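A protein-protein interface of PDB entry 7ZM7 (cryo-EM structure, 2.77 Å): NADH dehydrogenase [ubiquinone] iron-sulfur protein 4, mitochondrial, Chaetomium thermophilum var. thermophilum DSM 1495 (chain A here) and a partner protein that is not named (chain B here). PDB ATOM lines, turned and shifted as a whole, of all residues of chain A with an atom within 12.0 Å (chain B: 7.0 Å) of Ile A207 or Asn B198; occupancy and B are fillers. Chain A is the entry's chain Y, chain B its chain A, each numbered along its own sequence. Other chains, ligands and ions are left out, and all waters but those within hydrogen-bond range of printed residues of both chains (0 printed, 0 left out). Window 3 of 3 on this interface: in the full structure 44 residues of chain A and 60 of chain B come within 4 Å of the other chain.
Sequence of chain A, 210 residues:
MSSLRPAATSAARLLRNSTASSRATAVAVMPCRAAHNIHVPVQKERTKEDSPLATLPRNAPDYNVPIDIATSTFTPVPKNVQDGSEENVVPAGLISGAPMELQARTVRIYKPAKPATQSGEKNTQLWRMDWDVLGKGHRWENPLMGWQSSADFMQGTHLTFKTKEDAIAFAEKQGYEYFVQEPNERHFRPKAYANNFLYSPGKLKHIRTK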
ATOM      1  N   ASN A 195       4.187 -30.593  -1.369  1.00  0.00           N
ATOM      2  CA  ASN A 195       3.789 -30.857  -2.776  1.00  0.00           C
ATOM      3  C   ASN A 195       4.113 -29.647  -3.652  1.00  0.00           C
ATOM      4  O   ASN A 195       4.374 -29.851  -4.849  1.00  0.00           O
ATOM      5  CB  ASN A 195       2.300 -31.185  -2.883  1.00  0.00           C
ATOM      6  CG  ASN A 195       1.927 -32.487  -2.207  1.00  0.00           C
ATOM      7  OD1 ASN A 195       0.792 -32.663  -1.772  1.00  0.00           O
ATOM      8  ND2 ASN A 195       2.876 -33.405  -2.111  1.00  0.00           N
ATOM      9  N   ASN A 196       4.074 -28.444  -3.084  1.00  0.00           N
ATOM     10  CA  ASN A 196       4.348 -27.250  -3.866  1.00  0.00           C
ATOM     11  C   ASN A 196       5.679 -27.361  -4.592  1.00  0.00           C
ATOM     12  O   ASN A 196       5.916 -26.627  -5.552  1.00  0.00           O
ATOM     13  CB  ASN A 196       4.360 -26.006  -2.968  1.00  0.00           C
ATOM     14  CG  ASN A 196       3.018 -25.735  -2.284  1.00  0.00           C
ATOM     15  OD1 ASN A 196       2.134 -26.577  -2.262  1.00  0.00           O
ATOM     16  ND2 ASN A 196       2.887 -24.570  -1.692  1.00  0.00           N
ATOM     17  N   PHE A 197       6.550 -28.263  -4.155  1.00  0.00           N
ATOM     18  CA  PHE A 197       7.922 -28.367  -4.628  1.00  0.00           C
ATOM     19  C   PHE A 197       8.232 -29.791  -5.032  1.00  0.00           C
ATOM     20  O   PHE A 197       9.376 -30.228  -4.944  1.00  0.00           O
ATOM     21  CB  PHE A 197       8.903 -27.936  -3.554  1.00  0.00           C
ATOM     22  CG  PHE A 197       8.478 -26.727  -2.827  1.00  0.00           C
ATOM     23  CD1 PHE A 197       8.519 -25.495  -3.426  1.00  0.00           C
ATOM     24  CD2 PHE A 197       8.020 -26.826  -1.533  1.00  0.00           C
ATOM     25  CE1 PHE A 197       8.126 -24.403  -2.753  1.00  0.00           C
ATOM     26  CE2 PHE A 197       7.623 -25.725  -0.867  1.00  0.00           C
ATOM     27  CZ  PHE A 197       7.678 -24.517  -1.474  1.00  0.00           C
ATOM     28  N   LEU A 198       7.215 -30.544  -5.417  1.00  0.00           N
ATOM     29  CA  LEU A 198       7.443 -31.869  -5.948  1.00  0.00           C
ATOM     30  C   LEU A 198       8.218 -31.764  -7.256  1.00  0.00           C
ATOM     31  O   LEU A 198       8.161 -30.755  -7.956  1.00  0.00           O
ATOM     32  CB  LEU A 198       6.108 -32.588  -6.128  1.00  0.00           C
ATOM     33  CG  LEU A 198       6.065 -34.060  -6.508  1.00  0.00           C
ATOM     34  CD1 LEU A 198       4.779 -34.660  -5.985  1.00  0.00           C
ATOM     35  CD2 LEU A 198       6.104 -34.234  -8.003  1.00  0.00           C
ATOM     36  N   TYR A 199       8.993 -32.809  -7.542  1.00  0.00           N
ATOM     37  CA  TYR A 199       9.898 -32.852  -8.682  1.00  0.00           C
ATOM     38  C   TYR A 199       9.200 -33.399  -9.917  1.00  0.00           C
ATOM     39  O   TYR A 199       8.533 -34.431  -9.852  1.00  0.00           O
ATOM     40  CB  TYR A 199      11.097 -33.723  -8.331  1.00  0.00           C
ATOM     41  CG  TYR A 199      11.920 -34.215  -9.498  1.00  0.00           C
ATOM     42  CD1 TYR A 199      12.847 -33.399 -10.106  1.00  0.00           C
ATOM     43  CD2 TYR A 199      11.774 -35.499  -9.977  1.00  0.00           C
ATOM     44  CE1 TYR A 199      13.605 -33.842 -11.142  1.00  0.00           C
ATOM     45  CE2 TYR A 199      12.524 -35.949 -11.021  1.00  0.00           C
ATOM     46  CZ  TYR A 199      13.443 -35.114 -11.597  1.00  0.00           C
ATOM     47  OH  TYR A 199      14.204 -35.551 -12.649  1.00  0.00           O
ATOM     48  N   SER A 200       9.386 -32.738 -11.048  1.00  0.00           N
ATOM     49  CA  SER A 200       8.811 -33.200 -12.304  1.00  0.00           C
ATOM     50  C   SER A 200       9.895 -33.829 -13.163  1.00  0.00           C
ATOM     51  O   SER A 200      10.780 -33.111 -13.649  1.00  0.00           O
ATOM     52  CB  SER A 200       8.162 -32.046 -13.061  1.00  0.00           C
ATOM     53  OG  SER A 200       9.117 -31.430 -13.899  1.00  0.00           O
ATOM     54  N   GLY A 202       9.464 -34.918 -16.178  1.00  0.00           N
ATOM     55  CA  GLY A 202       9.192 -34.472 -17.524  1.00  0.00           C
ATOM     56  C   GLY A 202       8.828 -33.008 -17.602  1.00  0.00           C
ATOM     57  O   GLY A 202       9.214 -32.203 -16.747  1.00  0.00           O
ATOM     58  N   LYS A 203       8.063 -32.661 -18.638  1.00  0.00           N
ATOM     59  CA  LYS A 203       7.639 -31.288 -18.866  1.00  0.00           C
ATOM     60  C   LYS A 203       6.917 -30.733 -17.647  1.00  0.00           C
ATOM     61  O   LYS A 203       6.218 -31.448 -16.928  1.00  0.00           O
ATOM     62  CB  LYS A 203       6.727 -31.217 -20.086  1.00  0.00           C
ATOM     63  CG  LYS A 203       6.376 -29.808 -20.524  1.00  0.00           C
ATOM     64  CD  LYS A 203       7.596 -29.061 -21.025  1.00  0.00           C
ATOM     65  CE  LYS A 203       7.208 -28.009 -22.054  1.00  0.00           C
ATOM     66  NZ  LYS A 203       8.383 -27.497 -22.812  1.00  0.00           N
ATOM     67  N   LEU A 204       7.099 -29.439 -17.408  1.00  0.00           N
ATOM     68  CA  LEU A 204       6.643 -28.867 -16.152  1.00  0.00           C
ATOM     69  C   LEU A 204       5.128 -28.741 -16.099  1.00  0.00           C
ATOM     70  O   LEU A 204       4.506 -29.088 -15.092  1.00  0.00           O
ATOM     71  CB  LEU A 204       7.330 -27.530 -15.912  1.00  0.00           C
ATOM     72  CG  LEU A 204       8.585 -27.817 -15.079  1.00  0.00           C
ATOM     73  CD1 LEU A 204       9.442 -26.591 -14.855  1.00  0.00           C
ATOM     74  CD2 LEU A 204       8.171 -28.399 -13.769  1.00  0.00           C
ATOM     75  N   LYS A 205       4.519 -28.240 -17.157  1.00  0.00           N
ATOM     76  CA  LYS A 205       3.072 -28.094 -17.281  1.00  0.00           C
ATOM     77  C   LYS A 205       2.466 -27.221 -16.190  1.00  0.00           C
ATOM     78  O   LYS A 205       1.245 -27.158 -16.057  1.00  0.00           O
ATOM     79  CB  LYS A 205       2.377 -29.459 -17.348  1.00  0.00           C
ATOM     80  CG  LYS A 205       1.920 -30.107 -16.059  1.00  0.00           C
ATOM     81  CD  LYS A 205       1.315 -31.436 -16.409  1.00  0.00           C
ATOM     82  CE  LYS A 205       0.775 -32.133 -15.205  1.00  0.00           C
ATOM     83  NZ  LYS A 205       0.002 -33.357 -15.562  1.00  0.00           N
ATOM     84  N   HIS A 206       3.337 -26.529 -15.453  1.00  0.00           N
ATOM     85  CA  HIS A 206       2.890 -25.608 -14.385  1.00  0.00           C
ATOM     86  C   HIS A 206       4.110 -24.873 -13.842  1.00  0.00           C
ATOM     87  O   HIS A 206       5.121 -25.544 -13.574  1.00  0.00           O
ATOM     88  CB  HIS A 206       2.214 -26.366 -13.241  1.00  0.00           C
ATOM     89  CG  HIS A 206       1.534 -25.446 -12.293  1.00  0.00           C
ATOM     90  ND1 HIS A 206       1.836 -25.417 -10.950  1.00  0.00           N
ATOM     91  CD2 HIS A 206       0.601 -24.495 -12.503  1.00  0.00           C
ATOM     92  CE1 HIS A 206       1.099 -24.498 -10.365  1.00  0.00           C
ATOM     93  NE2 HIS A 206       0.336 -23.919 -11.297  1.00  0.00           N
ATOM     94  N   ILE A 207       4.025 -23.555 -13.712  1.00  0.00           N
ATOM     95  CA  ILE A 207       5.106 -22.778 -13.112  1.00  0.00           C
ATOM     96  C   ILE A 207       4.537 -22.170 -11.834  1.00  0.00           C
ATOM     97  O   ILE A 207       3.959 -21.082 -11.846  1.00  0.00           O
ATOM     98  CB  ILE A 207       5.664 -21.701 -14.045  1.00  0.00           C
ATOM     99  CG1 ILE A 207       6.166 -22.324 -15.344  1.00  0.00           C
ATOM    100  CG2 ILE A 207       6.795 -20.962 -13.376  1.00  0.00           C
ATOM    101  CD1 ILE A 207       7.265 -23.309 -15.169  1.00  0.00           C
ATOM    102  N   ARG A 208       4.691 -22.888 -10.729  1.00  0.00           N
ATOM    103  CA  ARG A 208       4.227 -22.451  -9.421  1.00  0.00           C
ATOM    104  C   ARG A 208       4.865 -21.117  -9.056  1.00  0.00           C
ATOM    105  O   ARG A 208       6.079 -20.944  -9.178  1.00  0.00           O
ATOM    106  CB  ARG A 208       4.608 -23.537  -8.418  1.00  0.00           C
ATOM    107  CG  ARG A 208       4.268 -23.339  -6.961  1.00  0.00           C
ATOM    108  CD  ARG A 208       2.806 -23.364  -6.639  1.00  0.00           C
ATOM    109  NE  ARG A 208       2.224 -24.671  -6.887  1.00  0.00           N
ATOM    110  CZ  ARG A 208       0.920 -24.903  -6.877  1.00  0.00           C
ATOM    111  NH1 ARG A 208       0.445 -26.116  -7.118  1.00  0.00           N
ATOM    112  NH2 ARG A 208       0.091 -23.922  -6.577  1.00  0.00           N
ATOM    113  N   THR A 209       4.054 -20.164  -8.609  1.00  0.00           N
ATOM    114  CA  THR A 209       4.555 -18.825  -8.302  1.00  0.00           C
ATOM    115  C   THR A 209       4.230 -18.388  -6.889  1.00  0.00           C
ATOM    116  O   THR A 209       3.909 -17.222  -6.656  1.00  0.00           O
ATOM    117  CB  THR A 209       4.015 -17.780  -9.265  1.00  0.00           C
ATOM    118  OG1 THR A 209       4.468 -16.491  -8.839  1.00  0.00           O
ATOM    119  CG2 THR A 209       2.509 -17.792  -9.298  1.00  0.00           C
ATOM    120  N   LYS A 210       4.342 -19.283  -5.920  1.00  0.00           N
ATOM    121  CA  LYS A 210       4.061 -18.927  -4.532  1.00  0.00           C
ATOM    122  C   LYS A 210       2.662 -18.341  -4.388  1.00  0.00           C
ATOM    123  O   LYS A 210       1.794 -18.545  -5.236  1.00  0.00           O
ATOM    124  CB  LYS A 210       5.081 -17.925  -4.006  1.00  0.00           C
ATOM    125  CG  LYS A 210       6.473 -18.455  -3.869  1.00  0.00           C
ATOM    126  CD  LYS A 210       6.726 -18.978  -2.503  1.00  0.00           C
ATOM    127  CE  LYS A 210       8.207 -19.040  -2.239  1.00  0.00           C
ATOM    128  NZ  LYS A 210       8.518 -19.866  -1.078  1.00  0.00           N
ATOM    129  OXT LYS A 210       2.372 -17.638  -3.427  1.00  0.00           O
ATOM    130  N   CYS B 193      -4.985 -14.798  -4.376  1.00  0.00           N
ATOM    131  CA  CYS B 193      -5.451 -14.562  -5.767  1.00  0.00           C
ATOM    132  C   CYS B 193      -4.376 -14.998  -6.759  1.00  0.00           C
ATOM    133  O   CYS B 193      -4.748 -15.542  -7.797  1.00  0.00           O
ATOM    134  CB  CYS B 193      -5.649 -13.071  -5.998  1.00  0.00           C
ATOM    135  SG  CYS B 193      -4.261 -12.050  -5.429  1.00  0.00           S
ATOM    136  N   VAL B 194      -3.098 -14.759  -6.459  1.00  0.00           N
ATOM    137  CA  VAL B 194      -2.091 -15.262  -7.383  1.00  0.00           C
ATOM    138  C   VAL B 194      -2.114 -16.781  -7.417  1.00  0.00           C
ATOM    139  O   VAL B 194      -1.872 -17.396  -8.457  1.00  0.00           O
ATOM    140  CB  VAL B 194      -0.700 -14.731  -7.001  1.00  0.00           C
ATOM    141  CG1 VAL B 194       0.326 -15.194  -7.990  1.00  0.00           C
ATOM    142  CG2 VAL B 194      -0.695 -13.226  -6.903  1.00  0.00           C
ATOM    143  N   ARG B 195      -2.393 -17.410  -6.279  1.00  0.00           N
ATOM    144  CA  ARG B 195      -2.503 -18.857  -6.255  1.00  0.00           C
ATOM    145  C   ARG B 195      -3.743 -19.324  -7.004  1.00  0.00           C
ATOM    146  O   ARG B 195      -3.698 -20.324  -7.720  1.00  0.00           O
ATOM    147  CB  ARG B 195      -2.508 -19.353  -4.813  1.00  0.00           C
ATOM    148  CG  ARG B 195      -1.121 -19.512  -4.228  1.00  0.00           C
ATOM    149  CD  ARG B 195      -1.152 -19.948  -2.787  1.00  0.00           C
ATOM    150  NE  ARG B 195      -1.742 -18.930  -1.944  1.00  0.00           N
ATOM    151  CZ  ARG B 195      -2.460 -19.183  -0.866  1.00  0.00           C
ATOM    152  NH1 ARG B 195      -2.652 -20.424  -0.477  1.00  0.00           N
ATOM    153  NH2 ARG B 195      -2.972 -18.195  -0.169  1.00  0.00           N
ATOM    154  N   PHE B 196      -4.862 -18.622  -6.851  1.00  0.00           N
ATOM    155  CA  PHE B 196      -6.067 -19.006  -7.574  1.00  0.00           C
ATOM    156  C   PHE B 196      -5.913 -18.803  -9.074  1.00  0.00           C
ATOM    157  O   PHE B 196      -6.315 -19.657  -9.863  1.00  0.00           O
ATOM    158  CB  PHE B 196      -7.264 -18.218  -7.072  1.00  0.00           C
ATOM    159  CG  PHE B 196      -8.512 -18.499  -7.835  1.00  0.00           C
ATOM    160  CD1 PHE B 196      -9.290 -19.577  -7.512  1.00  0.00           C
ATOM    161  CD2 PHE B 196      -8.885 -17.711  -8.897  1.00  0.00           C
ATOM    162  CE1 PHE B 196     -10.409 -19.847  -8.203  1.00  0.00           C
ATOM    163  CE2 PHE B 196     -10.003 -17.991  -9.596  1.00  0.00           C
ATOM    164  CZ  PHE B 196     -10.763 -19.063  -9.251  1.00  0.00           C
ATOM    165  N   MET B 197      -5.347 -17.677  -9.490  1.00  0.00           N
ATOM    166  CA  MET B 197      -5.312 -17.375 -10.914  1.00  0.00           C
ATOM    167  C   MET B 197      -4.293 -18.246 -11.628  1.00  0.00           C
ATOM    168  O   MET B 197      -4.491 -18.592 -12.791  1.00  0.00           O
ATOM    169  CB  MET B 197      -5.011 -15.889 -11.127  1.00  0.00           C
ATOM    170  CG  MET B 197      -6.233 -14.998 -10.972  1.00  0.00           C
ATOM    171  SD  MET B 197      -7.492 -15.048 -12.251  1.00  0.00           S
ATOM    172  CE  MET B 197      -6.535 -14.612 -13.669  1.00  0.00           C
ATOM    173  N   ASN B 198      -3.212 -18.616 -10.945  1.00  0.00           N
ATOM    174  CA  ASN B 198      -2.154 -19.416 -11.545  1.00  0.00           C
ATOM    175  C   ASN B 198      -2.465 -20.904 -11.535  1.00  0.00           C
ATOM    176  O   ASN B 198      -2.014 -21.632 -12.423  1.00  0.00           O
ATOM    177  CB  ASN B 198      -0.839 -19.171 -10.819  1.00  0.00           C
ATOM    178  CG  ASN B 198       0.341 -19.582 -11.624  1.00  0.00           C
ATOM    179  OD1 ASN B 198       0.385 -19.356 -12.821  1.00  0.00           O
ATOM    180  ND2 ASN B 198       1.304 -20.211 -10.985  1.00  0.00           N
ATOM    181  N   ASP B 199      -3.214 -21.379 -10.557  1.00  0.00           N
ATOM    182  CA  ASP B 199      -3.406 -22.803 -10.373  1.00  0.00           C
ATOM    183  C   ASP B 199      -4.801 -23.283 -10.728  1.00  0.00           C
ATOM    184  O   ASP B 199      -4.942 -24.327 -11.352  1.00  0.00           O
ATOM    185  CB  ASP B 199      -3.079 -23.186  -8.929  1.00  0.00           C
ATOM    186  CG  ASP B 199      -1.775 -22.565  -8.443  1.00  0.00           C
ATOM    187  OD1 ASP B 199      -0.785 -22.525  -9.208  1.00  0.00           O
ATOM    188  OD2 ASP B 199      -1.720 -22.111  -7.284  1.00  0.00           O
ATOM    189  N   ILE B 200      -5.839 -22.554 -10.359  1.00  0.00           N
ATOM    190  CA  ILE B 200      -7.196 -22.979 -10.665  1.00  0.00           C
ATOM    191  C   ILE B 200      -7.657 -22.415 -11.997  1.00  0.00           C
ATOM    192  O   ILE B 200      -8.208 -23.132 -12.829  1.00  0.00           O
ATOM    193  CB  ILE B 200      -8.149 -22.599  -9.510  1.00  0.00           C
ATOM    194  CG1 ILE B 200      -7.754 -23.343  -8.242  1.00  0.00           C
ATOM    195  CG2 ILE B 200      -9.568 -22.938  -9.847  1.00  0.00           C
ATOM    196  CD1 ILE B 200      -6.767 -22.634  -7.407  1.00  0.00           C
ATOM    197  N   ALA B 201      -7.416 -21.137 -12.240  1.00  0.00           N
ATOM    198  CA  ALA B 201      -7.872 -20.517 -13.470  1.00  0.00           C
ATOM    199  C   ALA B 201      -6.921 -20.738 -14.634  1.00  0.00           C
ATOM    200  O   ALA B 201      -7.334 -20.571 -15.784  1.00  0.00           O
ATOM    201  CB  ALA B 201      -8.088 -19.024 -13.254  1.00  0.00           C
ATOM    202  N   GLY B 202      -5.674 -21.119 -14.377  1.00  0.00           N
ATOM    203  CA  GLY B 202      -4.736 -21.300 -15.462  1.00  0.00           C
ATOM    204  C   GLY B 202      -4.462 -20.032 -16.226  1.00  0.00           C
ATOM    205  O   GLY B 202      -4.242 -20.077 -17.438  1.00  0.00           O
ATOM    206  N   ALA B 203      -4.454 -18.895 -15.535  1.00  0.00           N
ATOM    207  CA  ALA B 203      -4.314 -17.576 -16.141  1.00  0.00           C
ATOM    208  C   ALA B 203      -3.210 -16.831 -15.413  1.00  0.00           C
ATOM    209  O   ALA B 203      -3.478 -16.030 -14.511  1.00  0.00           O
ATOM    210  CB  ALA B 203      -5.627 -16.812 -16.086  1.00  0.00           C
ATOM    211  N   PRO B 204      -1.971 -17.036 -15.799  1.00  0.00           N
ATOM    212  CA  PRO B 204      -0.820 -16.627 -14.985  1.00  0.00           C
ATOM    213  C   PRO B 204      -0.362 -15.179 -15.161  1.00  0.00           C
ATOM    214  O   PRO B 204       0.826 -14.883 -15.150  1.00  0.00           O
ATOM    215  CB  PRO B 204       0.264 -17.602 -15.450  1.00  0.00           C
ATOM    216  CG  PRO B 204      -0.065 -17.810 -16.879  1.00  0.00           C
ATOM    217  CD  PRO B 204      -1.540 -17.690 -17.044  1.00  0.00           C
ATOM    218  N   GLU B 205      -1.310 -14.265 -15.285  1.00  0.00           N
ATOM    219  CA  GLU B 205      -0.963 -12.875 -15.544  1.00  0.00           C
ATOM    220  C   GLU B 205      -0.850 -12.043 -14.280  1.00  0.00           C
ATOM    221  O   GLU B 205      -0.195 -11.002 -14.288  1.00  0.00           O
ATOM    222  CB  GLU B 205      -1.986 -12.235 -16.482  1.00  0.00           C
ATOM    223  CG  GLU B 205      -1.902 -12.706 -17.907  1.00  0.00           C
ATOM    224  CD  GLU B 205      -2.252 -14.176 -18.082  1.00  0.00           C
ATOM    225  OE1 GLU B 205      -3.349 -14.584 -17.655  1.00  0.00           O
ATOM    226  OE2 GLU B 205      -1.439 -14.916 -18.672  1.00  0.00           O
ATOM    227  N   LEU B 206      -1.483 -12.478 -13.207  1.00  0.00           N
ATOM    228  CA  LEU B 206      -1.332 -11.862 -11.907  1.00  0.00           C
ATOM    229  C   LEU B 206      -0.068 -12.381 -11.237  1.00  0.00           C
ATOM    230  O   LEU B 206       0.236 -13.571 -11.300  1.00  0.00           O
ATOM    231  CB  LEU B 206      -2.562 -12.167 -11.061  1.00  0.00           C
ATOM    232  CG  LEU B 206      -2.887 -11.252  -9.900  1.00  0.00           C
ATOM    233  CD1 LEU B 206      -3.167  -9.849 -10.404  1.00  0.00           C
ATOM    234  CD2 LEU B 206      -4.086 -11.819  -9.188  1.00  0.00           C
ATOM    235  N   ARG B 433      -8.584 -29.395 -14.942  1.00  0.00           N
ATOM    236  CA  ARG B 433      -7.201 -28.952 -14.840  1.00  0.00           C
ATOM    237  C   ARG B 433      -6.605 -29.297 -13.486  1.00  0.00           C
ATOM    238  O   ARG B 433      -5.414 -29.592 -13.382  1.00  0.00           O
ATOM    239  CB  ARG B 433      -7.125 -27.450 -15.090  1.00  0.00           C
ATOM    240  CG  ARG B 433      -5.791 -26.846 -14.796  1.00  0.00           C
ATOM    241  CD  ARG B 433      -5.862 -25.354 -14.786  1.00  0.00           C
ATOM    242  NE  ARG B 433      -4.649 -24.805 -14.206  1.00  0.00           N
ATOM    243  CZ  ARG B 433      -3.591 -24.460 -14.912  1.00  0.00           C
ATOM    244  NH1 ARG B 433      -3.612 -24.605 -16.218  1.00  0.00           N
ATOM    245  NH2 ARG B 433      -2.524 -23.988 -14.318  1.00  0.00           N
ATOM    246  N   LEU B 437      -3.215 -31.300 -13.223  1.00  0.00           N
ATOM    247  CA  LEU B 437      -2.001 -30.731 -12.668  1.00  0.00           C
ATOM    248  C   LEU B 437      -1.399 -31.628 -11.603  1.00  0.00           C
ATOM    249  O   LEU B 437      -0.223 -31.476 -11.270  1.00  0.00           O
ATOM    250  CB  LEU B 437      -2.291 -29.342 -12.089  1.00  0.00           C
ATOM    251  CG  LEU B 437      -2.354 -28.111 -12.992  1.00  0.00           C
ATOM    252  CD1 LEU B 437      -2.703 -26.895 -12.179  1.00  0.00           C
ATOM    253  CD2 LEU B 437      -1.050 -27.915 -13.693  1.00  0.00           C
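O of Ile A207 lies within hydrogen-bond range of ND2 of Asn B198.
NE2 of His A206 lies within hydrogen-bond range of OD1 of Asp B199, at 2.8 Å.
NH2 of Arg A208 is in salt-bridge range of OD2 of Asp B199 (2.7 Å).
NE2 of His A206 sits at hydrogen-bond distance from O of Asn B198, 3.5 Å away.
The backbone carbonyl oxygen of Arg B195 lies close to the side-chain carboxylate of Asp B199 (2.7 Å).
NH2 of Arg B433 lies within hydrogen-bond range of O of Asn B198 (3.1 Å).
The backbone carbonyl oxygen (O) of Asp B199 sits at hydrogen-bond distance from the guanidinium group (NE) of Arg B433 (2.9 Å).
Lys A205 touches Leu B437.
CD2 of His A206 touches NH2 of Arg B433, at 3.6 Å.
His A206 touches Leu B437.
Thr A209 touches Val B194 (CG2 to CG1, 3.6 Å).
Asn B198 touches Thr A209.
CG of Arg B195 touches O of Lys A210, 3.2 Å away.
Of the printed residues of chain B, His A206 touches Asn B198 (3.5 Å), Asp B199 (2.8 Å), Arg B433 (3.6 Å) and Leu B437 (3.6 Å).
Ile A207 touches just one residue of chain B: Asn B198 (2.9 Å).
Of the printed residues of chain B, Arg A208 touches Asp B199.
Printed residues of chain B within 4 Å of Thr A209: Val B194 and Asn B198.
Of chain A, only Thr A209 comes within 4 Å of Val B194.
Of the printed residues of chain A, Asn B198 touches His A206, Ile A207 and Thr A209.
No residue of chain A comes within 4 Å of Ile B200.
No residue of chain A comes within 4 Å of Gly B202.
No residue of chain A comes within 4 Å of Ala B203.
No residue of chain A comes within 4 Å of Pro B204.
Printed residues of chain A within 4 Å of Arg B433: His A206 (3.6 Å).
Printed residues of chain A within 4 Å of Leu B437: Lys A205 and His A206.
The nearest residue of chain B that does not touch Ile A207 is Asp B199 (5.6 Å).
Hydrophobic or aromatic side chains of chain A within 4 Å of the printed part of chain B: His A206.
Hydrophobic or aromatic side chains of chain B within 4 Å of the printed part of chain A: Val B194 and Leu B437.
Among the printed residues, 10 pairs touch across the chains.
Among the printed residues, Asp or Glu carboxylates within 4 Å of a Lys or Arg side-chain nitrogen of the other chain: Arg A208 with Asp B199 (2.7 Å).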
